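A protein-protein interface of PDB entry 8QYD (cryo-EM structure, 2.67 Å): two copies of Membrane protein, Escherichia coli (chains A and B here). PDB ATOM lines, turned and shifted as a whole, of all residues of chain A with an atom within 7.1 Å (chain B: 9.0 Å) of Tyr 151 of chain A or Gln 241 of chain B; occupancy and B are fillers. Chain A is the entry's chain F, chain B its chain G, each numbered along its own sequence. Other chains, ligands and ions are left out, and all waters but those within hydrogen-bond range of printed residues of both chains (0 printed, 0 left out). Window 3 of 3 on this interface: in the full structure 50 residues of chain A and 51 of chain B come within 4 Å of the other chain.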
ATOM      1  N   ALA A 100     -16.243  -3.982  -4.596  1.00  0.00           N
ATOM      2  CA  ALA A 100     -16.390  -3.719  -6.018  1.00  0.00           C
ATOM      3  C   ALA A 100     -15.967  -4.943  -6.823  1.00  0.00           C
ATOM      4  O   ALA A 100     -15.471  -5.935  -6.285  1.00  0.00           O
ATOM      5  CB  ALA A 100     -15.568  -2.493  -6.430  1.00  0.00           C
ATOM      6  N   HIS A 101     -16.179  -4.862  -8.134  1.00  0.00           N
ATOM      7  CA  HIS A 101     -15.806  -5.960  -9.016  1.00  0.00           C
ATOM      8  C   HIS A 101     -14.294  -6.149  -9.026  1.00  0.00           C
ATOM      9  O   HIS A 101     -13.531  -5.178  -9.042  1.00  0.00           O
ATOM     10  CB  HIS A 101     -16.317  -5.700 -10.433  1.00  0.00           C
ATOM     11  CG  HIS A 101     -15.767  -6.644 -11.456  1.00  0.00           C
ATOM     12  ND1 HIS A 101     -14.671  -6.340 -12.235  1.00  0.00           N
ATOM     13  CD2 HIS A 101     -16.159  -7.886 -11.825  1.00  0.00           C
ATOM     14  CE1 HIS A 101     -14.413  -7.354 -13.042  1.00  0.00           C
ATOM     15  NE2 HIS A 101     -15.300  -8.304 -12.814  1.00  0.00           N
ATOM     16  N   ASN A 102     -13.868  -7.414  -9.010  1.00  0.00           N
ATOM     17  CA  ASN A 102     -12.449  -7.778  -9.009  1.00  0.00           C
ATOM     18  C   ASN A 102     -11.714  -7.150  -7.825  1.00  0.00           C
ATOM     19  O   ASN A 102     -10.555  -6.747  -7.932  1.00  0.00           O
ATOM     20  CB  ASN A 102     -11.777  -7.398 -10.331  1.00  0.00           C
ATOM     21  CG  ASN A 102     -10.586  -8.281 -10.654  1.00  0.00           C
ATOM     22  OD1 ASN A 102     -10.025  -8.936  -9.773  1.00  0.00           O
ATOM     23  ND2 ASN A 102     -10.192  -8.303 -11.922  1.00  0.00           N
ATOM     24  N   GLN A 103     -12.397  -7.065  -6.684  1.00  0.00           N
ATOM     25  CA  GLN A 103     -11.812  -6.551  -5.455  1.00  0.00           C
ATOM     26  C   GLN A 103     -11.943  -7.609  -4.370  1.00  0.00           C
ATOM     27  O   GLN A 103     -12.981  -8.269  -4.265  1.00  0.00           O
ATOM     28  CB  GLN A 103     -12.484  -5.246  -5.012  1.00  0.00           C
ATOM     29  CG  GLN A 103     -11.824  -4.597  -3.805  1.00  0.00           C
ATOM     30  CD  GLN A 103     -12.635  -3.451  -3.239  1.00  0.00           C
ATOM     31  OE1 GLN A 103     -13.566  -2.959  -3.877  1.00  0.00           O
ATOM     32  NE2 GLN A 103     -12.288  -3.018  -2.032  1.00  0.00           N
ATOM     33  N   THR A 143     -22.192 -12.744  -2.638  1.00  0.00           N
ATOM     34  CA  THR A 143     -21.920 -12.177  -3.950  1.00  0.00           C
ATOM     35  C   THR A 143     -23.185 -12.289  -4.794  1.00  0.00           C
ATOM     36  O   THR A 143     -24.031 -13.158  -4.564  1.00  0.00           O
ATOM     37  CB  THR A 143     -20.731 -12.890  -4.624  1.00  0.00           C
ATOM     38  OG1 THR A 143     -19.573 -12.771  -3.789  1.00  0.00           O
ATOM     39  CG2 THR A 143     -20.402 -12.269  -5.973  1.00  0.00           C
ATOM     40  N   ASP A 146     -25.231 -12.795 -10.619  1.00  0.00           N
ATOM     41  CA  ASP A 146     -24.800 -12.553 -11.988  1.00  0.00           C
ATOM     42  C   ASP A 146     -23.325 -12.905 -12.152  1.00  0.00           C
ATOM     43  O   ASP A 146     -22.609 -13.181 -11.187  1.00  0.00           O
ATOM     44  CB  ASP A 146     -25.047 -11.092 -12.379  1.00  0.00           C
ATOM     45  CG  ASP A 146     -26.437 -10.866 -12.935  1.00  0.00           C
ATOM     46  OD1 ASP A 146     -26.820 -11.575 -13.889  1.00  0.00           O
ATOM     47  OD2 ASP A 146     -27.148  -9.978 -12.419  1.00  0.00           O
ATOM     48  N   GLY A 147     -22.877 -12.893 -13.404  1.00  0.00           N
ATOM     49  CA  GLY A 147     -21.499 -13.206 -13.717  1.00  0.00           C
ATOM     50  C   GLY A 147     -21.220 -14.693 -13.646  1.00  0.00           C
ATOM     51  O   GLY A 147     -22.104 -15.525 -13.433  1.00  0.00           O
ATOM     52  N   SER A 148     -19.947 -15.031 -13.831  1.00  0.00           N
ATOM     53  CA  SER A 148     -19.524 -16.420 -13.739  1.00  0.00           C
ATOM     54  C   SER A 148     -19.621 -16.898 -12.296  1.00  0.00           C
ATOM     55  O   SER A 148     -19.153 -16.222 -11.375  1.00  0.00           O
ATOM     56  CB  SER A 148     -18.097 -16.577 -14.260  1.00  0.00           C
ATOM     57  OG  SER A 148     -17.655 -17.918 -14.147  1.00  0.00           O
ATOM     58  N   TYR A 149     -20.241 -18.064 -12.101  1.00  0.00           N
ATOM     59  CA  TYR A 149     -20.392 -18.604 -10.754  1.00  0.00           C
ATOM     60  C   TYR A 149     -19.039 -18.894 -10.120  1.00  0.00           C
ATOM     61  O   TYR A 149     -18.816 -18.585  -8.942  1.00  0.00           O
ATOM     62  CB  TYR A 149     -21.254 -19.868 -10.789  1.00  0.00           C
ATOM     63  CG  TYR A 149     -21.363 -20.578  -9.459  1.00  0.00           C
ATOM     64  CD1 TYR A 149     -22.316 -20.200  -8.523  1.00  0.00           C
ATOM     65  CD2 TYR A 149     -20.523 -21.640  -9.144  1.00  0.00           C
ATOM     66  CE1 TYR A 149     -22.421 -20.849  -7.307  1.00  0.00           C
ATOM     67  CE2 TYR A 149     -20.620 -22.294  -7.932  1.00  0.00           C
ATOM     68  CZ  TYR A 149     -21.571 -21.896  -7.017  1.00  0.00           C
ATOM     69  OH  TYR A 149     -21.672 -22.546  -5.809  1.00  0.00           O
ATOM     70  N   LEU A 150     -18.120 -19.484 -10.885  1.00  0.00           N
ATOM     71  CA  LEU A 150     -16.807 -19.797 -10.334  1.00  0.00           C
ATOM     72  C   LEU A 150     -16.011 -18.528 -10.057  1.00  0.00           C
ATOM     73  O   LEU A 150     -15.259 -18.464  -9.080  1.00  0.00           O
ATOM     74  CB  LEU A 150     -16.041 -20.727 -11.273  1.00  0.00           C
ATOM     75  CG  LEU A 150     -16.185 -22.217 -10.949  1.00  0.00           C
ATOM     76  CD1 LEU A 150     -15.576 -22.515  -9.588  1.00  0.00           C
ATOM     77  CD2 LEU A 150     -17.633 -22.679 -11.011  1.00  0.00           C
ATOM     78  N   TYR A 151     -16.168 -17.508 -10.905  1.00  0.00           N
ATOM     79  CA  TYR A 151     -15.540 -16.216 -10.641  1.00  0.00           C
ATOM     80  C   TYR A 151     -16.021 -15.639  -9.316  1.00  0.00           C
ATOM     81  O   TYR A 151     -15.216 -15.205  -8.484  1.00  0.00           O
ATOM     82  CB  TYR A 151     -15.835 -15.250 -11.791  1.00  0.00           C
ATOM     83  CG  TYR A 151     -15.286 -13.847 -11.613  1.00  0.00           C
ATOM     84  CD1 TYR A 151     -14.107 -13.615 -10.914  1.00  0.00           C
ATOM     85  CD2 TYR A 151     -15.953 -12.753 -12.148  1.00  0.00           C
ATOM     86  CE1 TYR A 151     -13.610 -12.336 -10.755  1.00  0.00           C
ATOM     87  CE2 TYR A 151     -15.463 -11.471 -11.993  1.00  0.00           C
ATOM     88  CZ  TYR A 151     -14.292 -11.268 -11.297  1.00  0.00           C
ATOM     89  OH  TYR A 151     -13.802  -9.993 -11.142  1.00  0.00           O
ATOM     90  N   ASN A 152     -17.340 -15.632  -9.102  1.00  0.00           N
ATOM     91  CA  ASN A 152     -17.887 -15.092  -7.863  1.00  0.00           C
ATOM     92  C   ASN A 152     -17.413 -15.893  -6.658  1.00  0.00           C
ATOM     93  O   ASN A 152     -17.037 -15.318  -5.628  1.00  0.00           O
ATOM     94  CB  ASN A 152     -19.414 -15.080  -7.932  1.00  0.00           C
ATOM     95  CG  ASN A 152     -19.937 -14.257  -9.092  1.00  0.00           C
ATOM     96  OD1 ASN A 152     -19.511 -13.122  -9.303  1.00  0.00           O
ATOM     97  ND2 ASN A 152     -20.862 -14.829  -9.853  1.00  0.00           N
ATOM     98  N   LEU A 153     -17.421 -17.224  -6.770  1.00  0.00           N
ATOM     99  CA  LEU A 153     -16.985 -18.060  -5.658  1.00  0.00           C
ATOM    100  C   LEU A 153     -15.519 -17.820  -5.326  1.00  0.00           C
ATOM    101  O   LEU A 153     -15.160 -17.660  -4.154  1.00  0.00           O
ATOM    102  CB  LEU A 153     -17.219 -19.533  -5.980  1.00  0.00           C
ATOM    103  CG  LEU A 153     -16.640 -20.481  -4.930  1.00  0.00           C
ATOM    104  CD1 LEU A 153     -17.626 -20.675  -3.792  1.00  0.00           C
ATOM    105  CD2 LEU A 153     -16.251 -21.808  -5.554  1.00  0.00           C
ATOM    106  N   HIS A 154     -14.655 -17.793  -6.346  1.00  0.00           N
ATOM    107  CA  HIS A 154     -13.235 -17.566  -6.107  1.00  0.00           C
ATOM    108  C   HIS A 154     -12.994 -16.189  -5.509  1.00  0.00           C
ATOM    109  O   HIS A 154     -12.181 -16.040  -4.591  1.00  0.00           O
ATOM    110  CB  HIS A 154     -12.448 -17.735  -7.406  1.00  0.00           C
ATOM    111  CG  HIS A 154     -10.992 -17.408  -7.275  1.00  0.00           C
ATOM    112  ND1 HIS A 154     -10.136 -18.128  -6.471  1.00  0.00           N
ATOM    113  CD2 HIS A 154     -10.243 -16.435  -7.846  1.00  0.00           C
ATOM    114  CE1 HIS A 154      -8.921 -17.615  -6.552  1.00  0.00           C
ATOM    115  NE2 HIS A 154      -8.959 -16.585  -7.378  1.00  0.00           N
ATOM    116  N   LEU A 155     -13.702 -15.172  -6.004  1.00  0.00           N
ATOM    117  CA  LEU A 155     -13.520 -13.823  -5.481  1.00  0.00           C
ATOM    118  C   LEU A 155     -13.931 -13.749  -4.014  1.00  0.00           C
ATOM    119  O   LEU A 155     -13.184 -13.228  -3.178  1.00  0.00           O
ATOM    120  CB  LEU A 155     -14.311 -12.827  -6.332  1.00  0.00           C
ATOM    121  CG  LEU A 155     -14.137 -11.321  -6.105  1.00  0.00           C
ATOM    122  CD1 LEU A 155     -14.431 -10.575  -7.397  1.00  0.00           C
ATOM    123  CD2 LEU A 155     -15.034 -10.800  -4.994  1.00  0.00           C
ATOM    124  N   SER A 156     -15.108 -14.284  -3.678  1.00  0.00           N
ATOM    125  CA  SER A 156     -15.572 -14.242  -2.293  1.00  0.00           C
ATOM    126  C   SER A 156     -14.663 -15.052  -1.375  1.00  0.00           C
ATOM    127  O   SER A 156     -14.388 -14.644  -0.239  1.00  0.00           O
ATOM    128  CB  SER A 156     -17.010 -14.749  -2.203  1.00  0.00           C
ATOM    129  OG  SER A 156     -17.902 -13.864  -2.857  1.00  0.00           O
ATOM    130  N   LEU A 157     -14.190 -16.208  -1.847  1.00  0.00           N
ATOM    131  CA  LEU A 157     -13.304 -17.025  -1.030  1.00  0.00           C
ATOM    132  C   LEU A 157     -11.971 -16.318  -0.814  1.00  0.00           C
ATOM    133  O   LEU A 157     -11.369 -16.419   0.262  1.00  0.00           O
ATOM    134  CB  LEU A 157     -13.104 -18.386  -1.695  1.00  0.00           C
ATOM    135  CG  LEU A 157     -12.314 -19.414  -0.897  1.00  0.00           C
ATOM    136  CD1 LEU A 157     -13.096 -19.728   0.364  1.00  0.00           C
ATOM    137  CD2 LEU A 157     -12.069 -20.670  -1.716  1.00  0.00           C
ATOM    138  N   GLN A 158     -11.501 -15.588  -1.828  1.00  0.00           N
ATOM    139  CA  GLN A 158     -10.306 -14.767  -1.674  1.00  0.00           C
ATOM    140  C   GLN A 158     -10.531 -13.656  -0.657  1.00  0.00           C
ATOM    141  O   GLN A 158      -9.633 -13.331   0.126  1.00  0.00           O
ATOM    142  CB  GLN A 158      -9.903 -14.188  -3.030  1.00  0.00           C
ATOM    143  CG  GLN A 158      -8.617 -13.390  -3.014  1.00  0.00           C
ATOM    144  CD  GLN A 158      -8.227 -12.884  -4.388  1.00  0.00           C
ATOM    145  OE1 GLN A 158      -7.185 -12.250  -4.555  1.00  0.00           O
ATOM    146  NE2 GLN A 158      -9.063 -13.160  -5.381  1.00  0.00           N
ATOM    147  N   PHE B 104      -3.731 -29.472  -4.948  1.00  0.00           N
ATOM    148  CA  PHE B 104      -5.170 -29.382  -4.734  1.00  0.00           C
ATOM    149  C   PHE B 104      -5.983 -30.111  -5.798  1.00  0.00           C
ATOM    150  O   PHE B 104      -7.199 -29.901  -5.882  1.00  0.00           O
ATOM    151  CB  PHE B 104      -5.599 -27.913  -4.651  1.00  0.00           C
ATOM    152  CG  PHE B 104      -5.319 -27.122  -5.898  1.00  0.00           C
ATOM    153  CD1 PHE B 104      -4.103 -26.483  -6.064  1.00  0.00           C
ATOM    154  CD2 PHE B 104      -6.271 -27.009  -6.896  1.00  0.00           C
ATOM    155  CE1 PHE B 104      -3.838 -25.751  -7.205  1.00  0.00           C
ATOM    156  CE2 PHE B 104      -6.012 -26.280  -8.039  1.00  0.00           C
ATOM    157  CZ  PHE B 104      -4.795 -25.648  -8.192  1.00  0.00           C
ATOM    158  N   GLN B 158      -8.165 -23.706  -1.686  1.00  0.00           N
ATOM    159  CA  GLN B 158      -7.913 -24.087  -3.069  1.00  0.00           C
ATOM    160  C   GLN B 158      -8.501 -25.457  -3.376  1.00  0.00           C
ATOM    161  O   GLN B 158      -8.996 -25.686  -4.483  1.00  0.00           O
ATOM    162  CB  GLN B 158      -6.412 -24.069  -3.358  1.00  0.00           C
ATOM    163  CG  GLN B 158      -5.848 -22.681  -3.609  1.00  0.00           C
ATOM    164  CD  GLN B 158      -4.405 -22.713  -4.076  1.00  0.00           C
ATOM    165  OE1 GLN B 158      -3.620 -23.560  -3.649  1.00  0.00           O
ATOM    166  NE2 GLN B 158      -4.049 -21.787  -4.959  1.00  0.00           N
ATOM    167  N   GLU B 161     -12.197 -24.845  -3.850  1.00  0.00           N
ATOM    168  CA  GLU B 161     -12.434 -24.180  -5.126  1.00  0.00           C
ATOM    169  C   GLU B 161     -12.231 -25.141  -6.290  1.00  0.00           C
ATOM    170  O   GLU B 161     -12.958 -25.078  -7.284  1.00  0.00           O
ATOM    171  CB  GLU B 161     -11.521 -22.961  -5.258  1.00  0.00           C
ATOM    172  CG  GLU B 161     -11.667 -22.220  -6.575  1.00  0.00           C
ATOM    173  CD  GLU B 161     -12.783 -21.199  -6.542  1.00  0.00           C
ATOM    174  OE1 GLU B 161     -13.100 -20.702  -5.441  1.00  0.00           O
ATOM    175  OE2 GLU B 161     -13.343 -20.895  -7.615  1.00  0.00           O
ATOM    176  N   TRP B 162     -11.249 -26.036  -6.183  1.00  0.00           N
ATOM    177  CA  TRP B 162     -11.039 -27.052  -7.208  1.00  0.00           C
ATOM    178  C   TRP B 162     -12.205 -28.027  -7.271  1.00  0.00           C
ATOM    179  O   TRP B 162     -12.613 -28.445  -8.359  1.00  0.00           O
ATOM    180  CB  TRP B 162      -9.723 -27.780  -6.945  1.00  0.00           C
ATOM    181  CG  TRP B 162      -9.413 -28.875  -7.913  1.00  0.00           C
ATOM    182  CD1 TRP B 162      -8.645 -28.784  -9.036  1.00  0.00           C
ATOM    183  CD2 TRP B 162      -9.816 -30.246  -7.812  1.00  0.00           C
ATOM    184  NE1 TRP B 162      -8.573 -30.006  -9.659  1.00  0.00           N
ATOM    185  CE2 TRP B 162      -9.279 -30.922  -8.925  1.00  0.00           C
ATOM    186  CE3 TRP B 162     -10.590 -30.966  -6.894  1.00  0.00           C
ATOM    187  CZ2 TRP B 162      -9.492 -32.280  -9.147  1.00  0.00           C
ATOM    188  CZ3 TRP B 162     -10.799 -32.314  -7.117  1.00  0.00           C
ATOM    189  CH2 TRP B 162     -10.247 -32.957  -8.231  1.00  0.00           C
ATOM    190  N   MET B 164     -15.336 -27.341  -6.458  1.00  0.00           N
ATOM    191  CA  MET B 164     -16.439 -26.620  -7.086  1.00  0.00           C
ATOM    192  C   MET B 164     -16.211 -26.428  -8.582  1.00  0.00           C
ATOM    193  O   MET B 164     -17.156 -26.544  -9.371  1.00  0.00           O
ATOM    194  CB  MET B 164     -16.652 -25.273  -6.402  1.00  0.00           C
ATOM    195  CG  MET B 164     -18.085 -24.777  -6.485  1.00  0.00           C
ATOM    196  SD  MET B 164     -19.239 -25.899  -5.672  1.00  0.00           S
ATOM    197  CE  MET B 164     -20.733 -25.585  -6.609  1.00  0.00           C
ATOM    198  N   CYS B 165     -14.975 -26.129  -8.987  1.00  0.00           N
ATOM    199  CA  CYS B 165     -14.638 -26.076 -10.406  1.00  0.00           C
ATOM    200  C   CYS B 165     -14.987 -27.390 -11.086  1.00  0.00           C
ATOM    201  O   CYS B 165     -15.753 -27.426 -12.054  1.00  0.00           O
ATOM    202  CB  CYS B 165     -13.144 -25.785 -10.576  1.00  0.00           C
ATOM    203  SG  CYS B 165     -12.625 -24.065 -10.456  1.00  0.00           S
ATOM    204  N   SER B 166     -14.469 -28.492 -10.544  1.00  0.00           N
ATOM    205  CA  SER B 166     -14.697 -29.809 -11.122  1.00  0.00           C
ATOM    206  C   SER B 166     -16.180 -30.130 -11.212  1.00  0.00           C
ATOM    207  O   SER B 166     -16.613 -30.820 -12.142  1.00  0.00           O
ATOM    208  CB  SER B 166     -13.975 -30.857 -10.279  1.00  0.00           C
ATOM    209  OG  SER B 166     -14.765 -31.257  -9.174  1.00  0.00           O
ATOM    210  N   LEU B 168     -18.457 -27.741 -11.679  1.00  0.00           N
ATOM    211  CA  LEU B 168     -19.061 -26.800 -12.616  1.00  0.00           C
ATOM    212  C   LEU B 168     -18.026 -26.103 -13.499  1.00  0.00           C
ATOM    213  O   LEU B 168     -18.027 -24.870 -13.600  1.00  0.00           O
ATOM    214  CB  LEU B 168     -19.898 -25.756 -11.871  1.00  0.00           C
ATOM    215  CG  LEU B 168     -21.106 -25.195 -12.623  1.00  0.00           C
ATOM    216  CD1 LEU B 168     -21.851 -26.316 -13.326  1.00  0.00           C
ATOM    217  CD2 LEU B 168     -22.029 -24.450 -11.672  1.00  0.00           C
ATOM    218  N   ASP B 169     -17.135 -26.858 -14.136  1.00  0.00           N
ATOM    219  CA  ASP B 169     -16.197 -26.303 -15.103  1.00  0.00           C
ATOM    220  C   ASP B 169     -16.532 -26.801 -16.503  1.00  0.00           C
ATOM    221  O   ASP B 169     -17.031 -27.914 -16.681  1.00  0.00           O
ATOM    222  CB  ASP B 169     -14.752 -26.672 -14.755  1.00  0.00           C
ATOM    223  CG  ASP B 169     -13.746 -26.081 -15.724  1.00  0.00           C
ATOM    224  OD1 ASP B 169     -14.007 -24.984 -16.260  1.00  0.00           O
ATOM    225  OD2 ASP B 169     -12.692 -26.714 -15.945  1.00  0.00           O
ATOM    226  N   LYS B 237     -20.459 -20.521 -20.721  1.00  0.00           N
ATOM    227  CA  LYS B 237     -19.916 -21.617 -19.933  1.00  0.00           C
ATOM    228  C   LYS B 237     -18.955 -21.103 -18.865  1.00  0.00           C
ATOM    229  O   LYS B 237     -18.239 -20.117 -19.059  1.00  0.00           O
ATOM    230  CB  LYS B 237     -19.204 -22.623 -20.836  1.00  0.00           C
ATOM    231  CG  LYS B 237     -20.115 -23.295 -21.848  1.00  0.00           C
ATOM    232  CD  LYS B 237     -21.174 -24.141 -21.161  1.00  0.00           C
ATOM    233  CE  LYS B 237     -20.568 -25.383 -20.532  1.00  0.00           C
ATOM    234  NZ  LYS B 237     -21.608 -26.258 -19.922  1.00  0.00           N
ATOM    235  N   GLU B 238     -18.948 -21.790 -17.726  1.00  0.00           N
ATOM    236  CA  GLU B 238     -18.078 -21.428 -16.618  1.00  0.00           C
ATOM    237  C   GLU B 238     -16.627 -21.769 -16.934  1.00  0.00           C
ATOM    238  O   GLU B 238     -16.333 -22.712 -17.672  1.00  0.00           O
ATOM    239  CB  GLU B 238     -18.510 -22.151 -15.340  1.00  0.00           C
ATOM    240  CG  GLU B 238     -19.876 -21.738 -14.813  1.00  0.00           C
ATOM    241  CD  GLU B 238     -19.904 -20.305 -14.320  1.00  0.00           C
ATOM    242  OE1 GLU B 238     -18.865 -19.826 -13.820  1.00  0.00           O
ATOM    243  OE2 GLU B 238     -20.967 -19.659 -14.432  1.00  0.00           O
ATOM    244  N   VAL B 239     -15.716 -20.983 -16.365  1.00  0.00           N
ATOM    245  CA  VAL B 239     -14.281 -21.189 -16.521  1.00  0.00           C
ATOM    246  C   VAL B 239     -13.647 -21.200 -15.137  1.00  0.00           C
ATOM    247  O   VAL B 239     -13.849 -20.269 -14.351  1.00  0.00           O
ATOM    248  CB  VAL B 239     -13.638 -20.100 -17.400  1.00  0.00           C
ATOM    249  CG1 VAL B 239     -12.129 -20.285 -17.460  1.00  0.00           C
ATOM    250  CG2 VAL B 239     -14.240 -20.114 -18.798  1.00  0.00           C
ATOM    251  N   CYS B 240     -12.888 -22.252 -14.840  1.00  0.00           N
ATOM    252  CA  CYS B 240     -12.192 -22.330 -13.564  1.00  0.00           C
ATOM    253  C   CYS B 240     -11.022 -21.353 -13.542  1.00  0.00           C
ATOM    254  O   CYS B 240     -10.314 -21.195 -14.541  1.00  0.00           O
ATOM    255  CB  CYS B 240     -11.693 -23.750 -13.310  1.00  0.00           C
ATOM    256  SG  CYS B 240     -10.994 -23.982 -11.662  1.00  0.00           S
ATOM    257  N   GLN B 241     -10.823 -20.696 -12.402  1.00  0.00           N
ATOM    258  CA  GLN B 241      -9.772 -19.696 -12.276  1.00  0.00           C
ATOM    259  C   GLN B 241      -8.563 -20.178 -11.484  1.00  0.00           C
ATOM    260  O   GLN B 241      -7.608 -19.412 -11.319  1.00  0.00           O
ATOM    261  CB  GLN B 241     -10.334 -18.423 -11.640  1.00  0.00           C
ATOM    262  CG  GLN B 241     -11.329 -17.710 -12.535  1.00  0.00           C
ATOM    263  CD  GLN B 241     -11.898 -16.459 -11.906  1.00  0.00           C
ATOM    264  OE1 GLN B 241     -11.609 -16.141 -10.753  1.00  0.00           O
ATOM    265  NE2 GLN B 241     -12.701 -15.732 -12.670  1.00  0.00           N
ATOM    266  N   LEU B 242      -8.575 -21.413 -10.990  1.00  0.00           N
ATOM    267  CA  LEU B 242      -7.376 -21.966 -10.380  1.00  0.00           C
ATOM    268  C   LEU B 242      -6.365 -22.348 -11.456  1.00  0.00           C
ATOM    269  O   LEU B 242      -6.712 -22.618 -12.610  1.00  0.00           O
ATOM    270  CB  LEU B 242      -7.714 -23.180  -9.516  1.00  0.00           C
ATOM    271  CG  LEU B 242      -8.433 -22.888  -8.199  1.00  0.00           C
ATOM    272  CD1 LEU B 242      -8.791 -24.181  -7.491  1.00  0.00           C
ATOM    273  CD2 LEU B 242      -7.580 -22.002  -7.304  1.00  0.00           C
ATOM    274  N   VAL B 243      -5.093 -22.371 -11.064  1.00  0.00           N
ATOM    275  CA  VAL B 243      -4.015 -22.675 -11.998  1.00  0.00           C
ATOM    276  C   VAL B 243      -3.943 -24.179 -12.238  1.00  0.00           C
ATOM    277  O   VAL B 243      -3.345 -24.927 -11.457  1.00  0.00           O
ATOM    278  CB  VAL B 243      -2.674 -22.098 -11.499  1.00  0.00           C
ATOM    279  CG1 VAL B 243      -2.691 -20.586 -11.608  1.00  0.00           C
ATOM    280  CG2 VAL B 243      -2.420 -22.483 -10.046  1.00  0.00           C
ATOM    281  N   MET B 244      -4.577 -24.634 -13.320  1.00  0.00           N
ATOM    282  CA  MET B 244      -4.533 -26.054 -13.659  1.00  0.00           C
ATOM    283  C   MET B 244      -3.123 -26.541 -13.976  1.00  0.00           C
ATOM    284  O   MET B 244      -2.707 -27.563 -13.402  1.00  0.00           O
ATOM    285  CB  MET B 244      -5.504 -26.339 -14.811  1.00  0.00           C
ATOM    286  CG  MET B 244      -5.600 -27.806 -15.198  1.00  0.00           C
ATOM    287  SD  MET B 244      -6.821 -28.103 -16.491  1.00  0.00           S
ATOM    288  CE  MET B 244      -6.597 -29.859 -16.770  1.00  0.00           C
ATOM    289  N   PRO B 245      -2.342 -25.896 -14.855  1.00  0.00           N
ATOM    290  CA  PRO B 245      -0.962 -26.365 -15.055  1.00  0.00           C
ATOM    291  C   PRO B 245      -0.090 -26.193 -13.824  1.00  0.00           C
ATOM    292  O   PRO B 245       0.844 -26.982 -13.631  1.00  0.00           O
ATOM    293  CB  PRO B 245      -0.462 -25.513 -16.229  1.00  0.00           C
ATOM    294  CG  PRO B 245      -1.292 -24.290 -16.186  1.00  0.00           C
ATOM    295  CD  PRO B 245      -2.642 -24.724 -15.701  1.00  0.00           C
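The backbone NH (N) of Tyr 149 of chain A lies within hydrogen-bond range of the side-chain carboxylate (OE1) of Glu 238 of chain B (2.8 Å). N of Leu 150 of chain A is in hydrogen-bond range of OE1 of Glu 238 of chain B (3.0 Å). N of His 154 of chain A sits close to OE1 of Glu 161 of chain B, at 3.4 Å. OG of Ser 148 of chain A sits close to OE1 of Glu 238 of chain B (2.3 Å). OE2 of Glu 161 of chain B sits close to O of Leu 150 of chain A.
NE2 of His 101 of chain A sits at hydrogen-bond distance from OH of Tyr 151 of chain A (2.8 Å). OH of Tyr 151 of chain A lies within hydrogen-bond range of N of Asn 102 of chain A, 3.3 Å away. The backbone carbonyl oxygen of Ser 148 of chain A sits at hydrogen-bond distance from the side-chain amide nitrogen of Asn 152 of chain A, at 2.7 Å. The side-chain sulfur (SG) of Cys 165 of chain B forms a disulfide with the side-chain sulfur (SG) of Cys 240 of chain B, 2.0 Å away.
Tyr 149 of chain A touches Met 164 of chain B (OH to CE, 3.3 Å). Cys 165 of chain B touches Leu 150 of chain A (SG to CD1, 3.4 Å). Leu 168 of chain B touches Leu 150 of chain A (O to CD2, 3.4 Å). Leu 150 of chain A touches Val 239 of chain B (CB to O, 3.8 Å). CD1 of Tyr 151 of chain A touches NE2 of Gln 241 of chain B, 3.1 Å away. Glu 161 of chain B touches Leu 153 of chain A. CD2 of Leu 153 of chain A touches CB of Met 164 of chain B, 3.6 Å away. Gln 241 of chain B touches His 154 of chain A (OE1 to CD2, 3.2 Å). Glu 161 of chain B touches Leu 157 of chain A (OE1 to CD2, 3.9 Å).
Of chain B, only Glu 238 comes within 4 Å of Ser 148 of chain A. Printed residues of chain B within 4 Å of Tyr 151 of chain A: Gln 241. No residue of chain B comes within 4 Å of Asn 152 of chain A. Phe 104 of chain B touches none of the printed residues of chain A. Of the printed residues of chain A, Glu 161 of chain B touches Leu 150, Leu 153, His 154 and Leu 157. Of the printed residues of chain A, Met 164 of chain B touches Tyr 149 and Leu 153. Of the printed residues of chain A, Leu 168 of chain B touches Leu 150. Printed residues of chain A within 4 Å of Glu 238 of chain B: Ser 148, Tyr 149 and Leu 150. Printed residues of chain A within 4 Å of Gln 241 of chain B: Tyr 151 and His 154. Val 243 of chain B touches none of the printed residues of chain A. The nearest residue of chain B that does not touch Tyr 151 of chain A is Glu 238 of chain B (4.6 Å). The nearest residue of chain A that does not touch Gln 241 of chain B is Leu 150 of chain A (4.6 Å).
Printed residues of chain A that touch a printed residue of chain B: Ser 148, Tyr 149, Leu 150, Tyr 151, Leu 153, His 154 and Leu 157. Hydrophobic or aromatic side chains of chain A within 4 Å of the printed part of chain B: Tyr 149, Leu 150, Tyr 151, Leu 153, His 154 and Leu 157. Of the 18 printed residues of chain B, 7 touch a printed residue of chain A. Along chain B the printed residues that touch a printed residue of chain A span positions 161 to 241. Among the printed residues, no Asp or Glu carboxylate lies within 4 Å of a Lys or Arg side-chain nitrogen of the other chain.
Position printed for both chains: 158.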
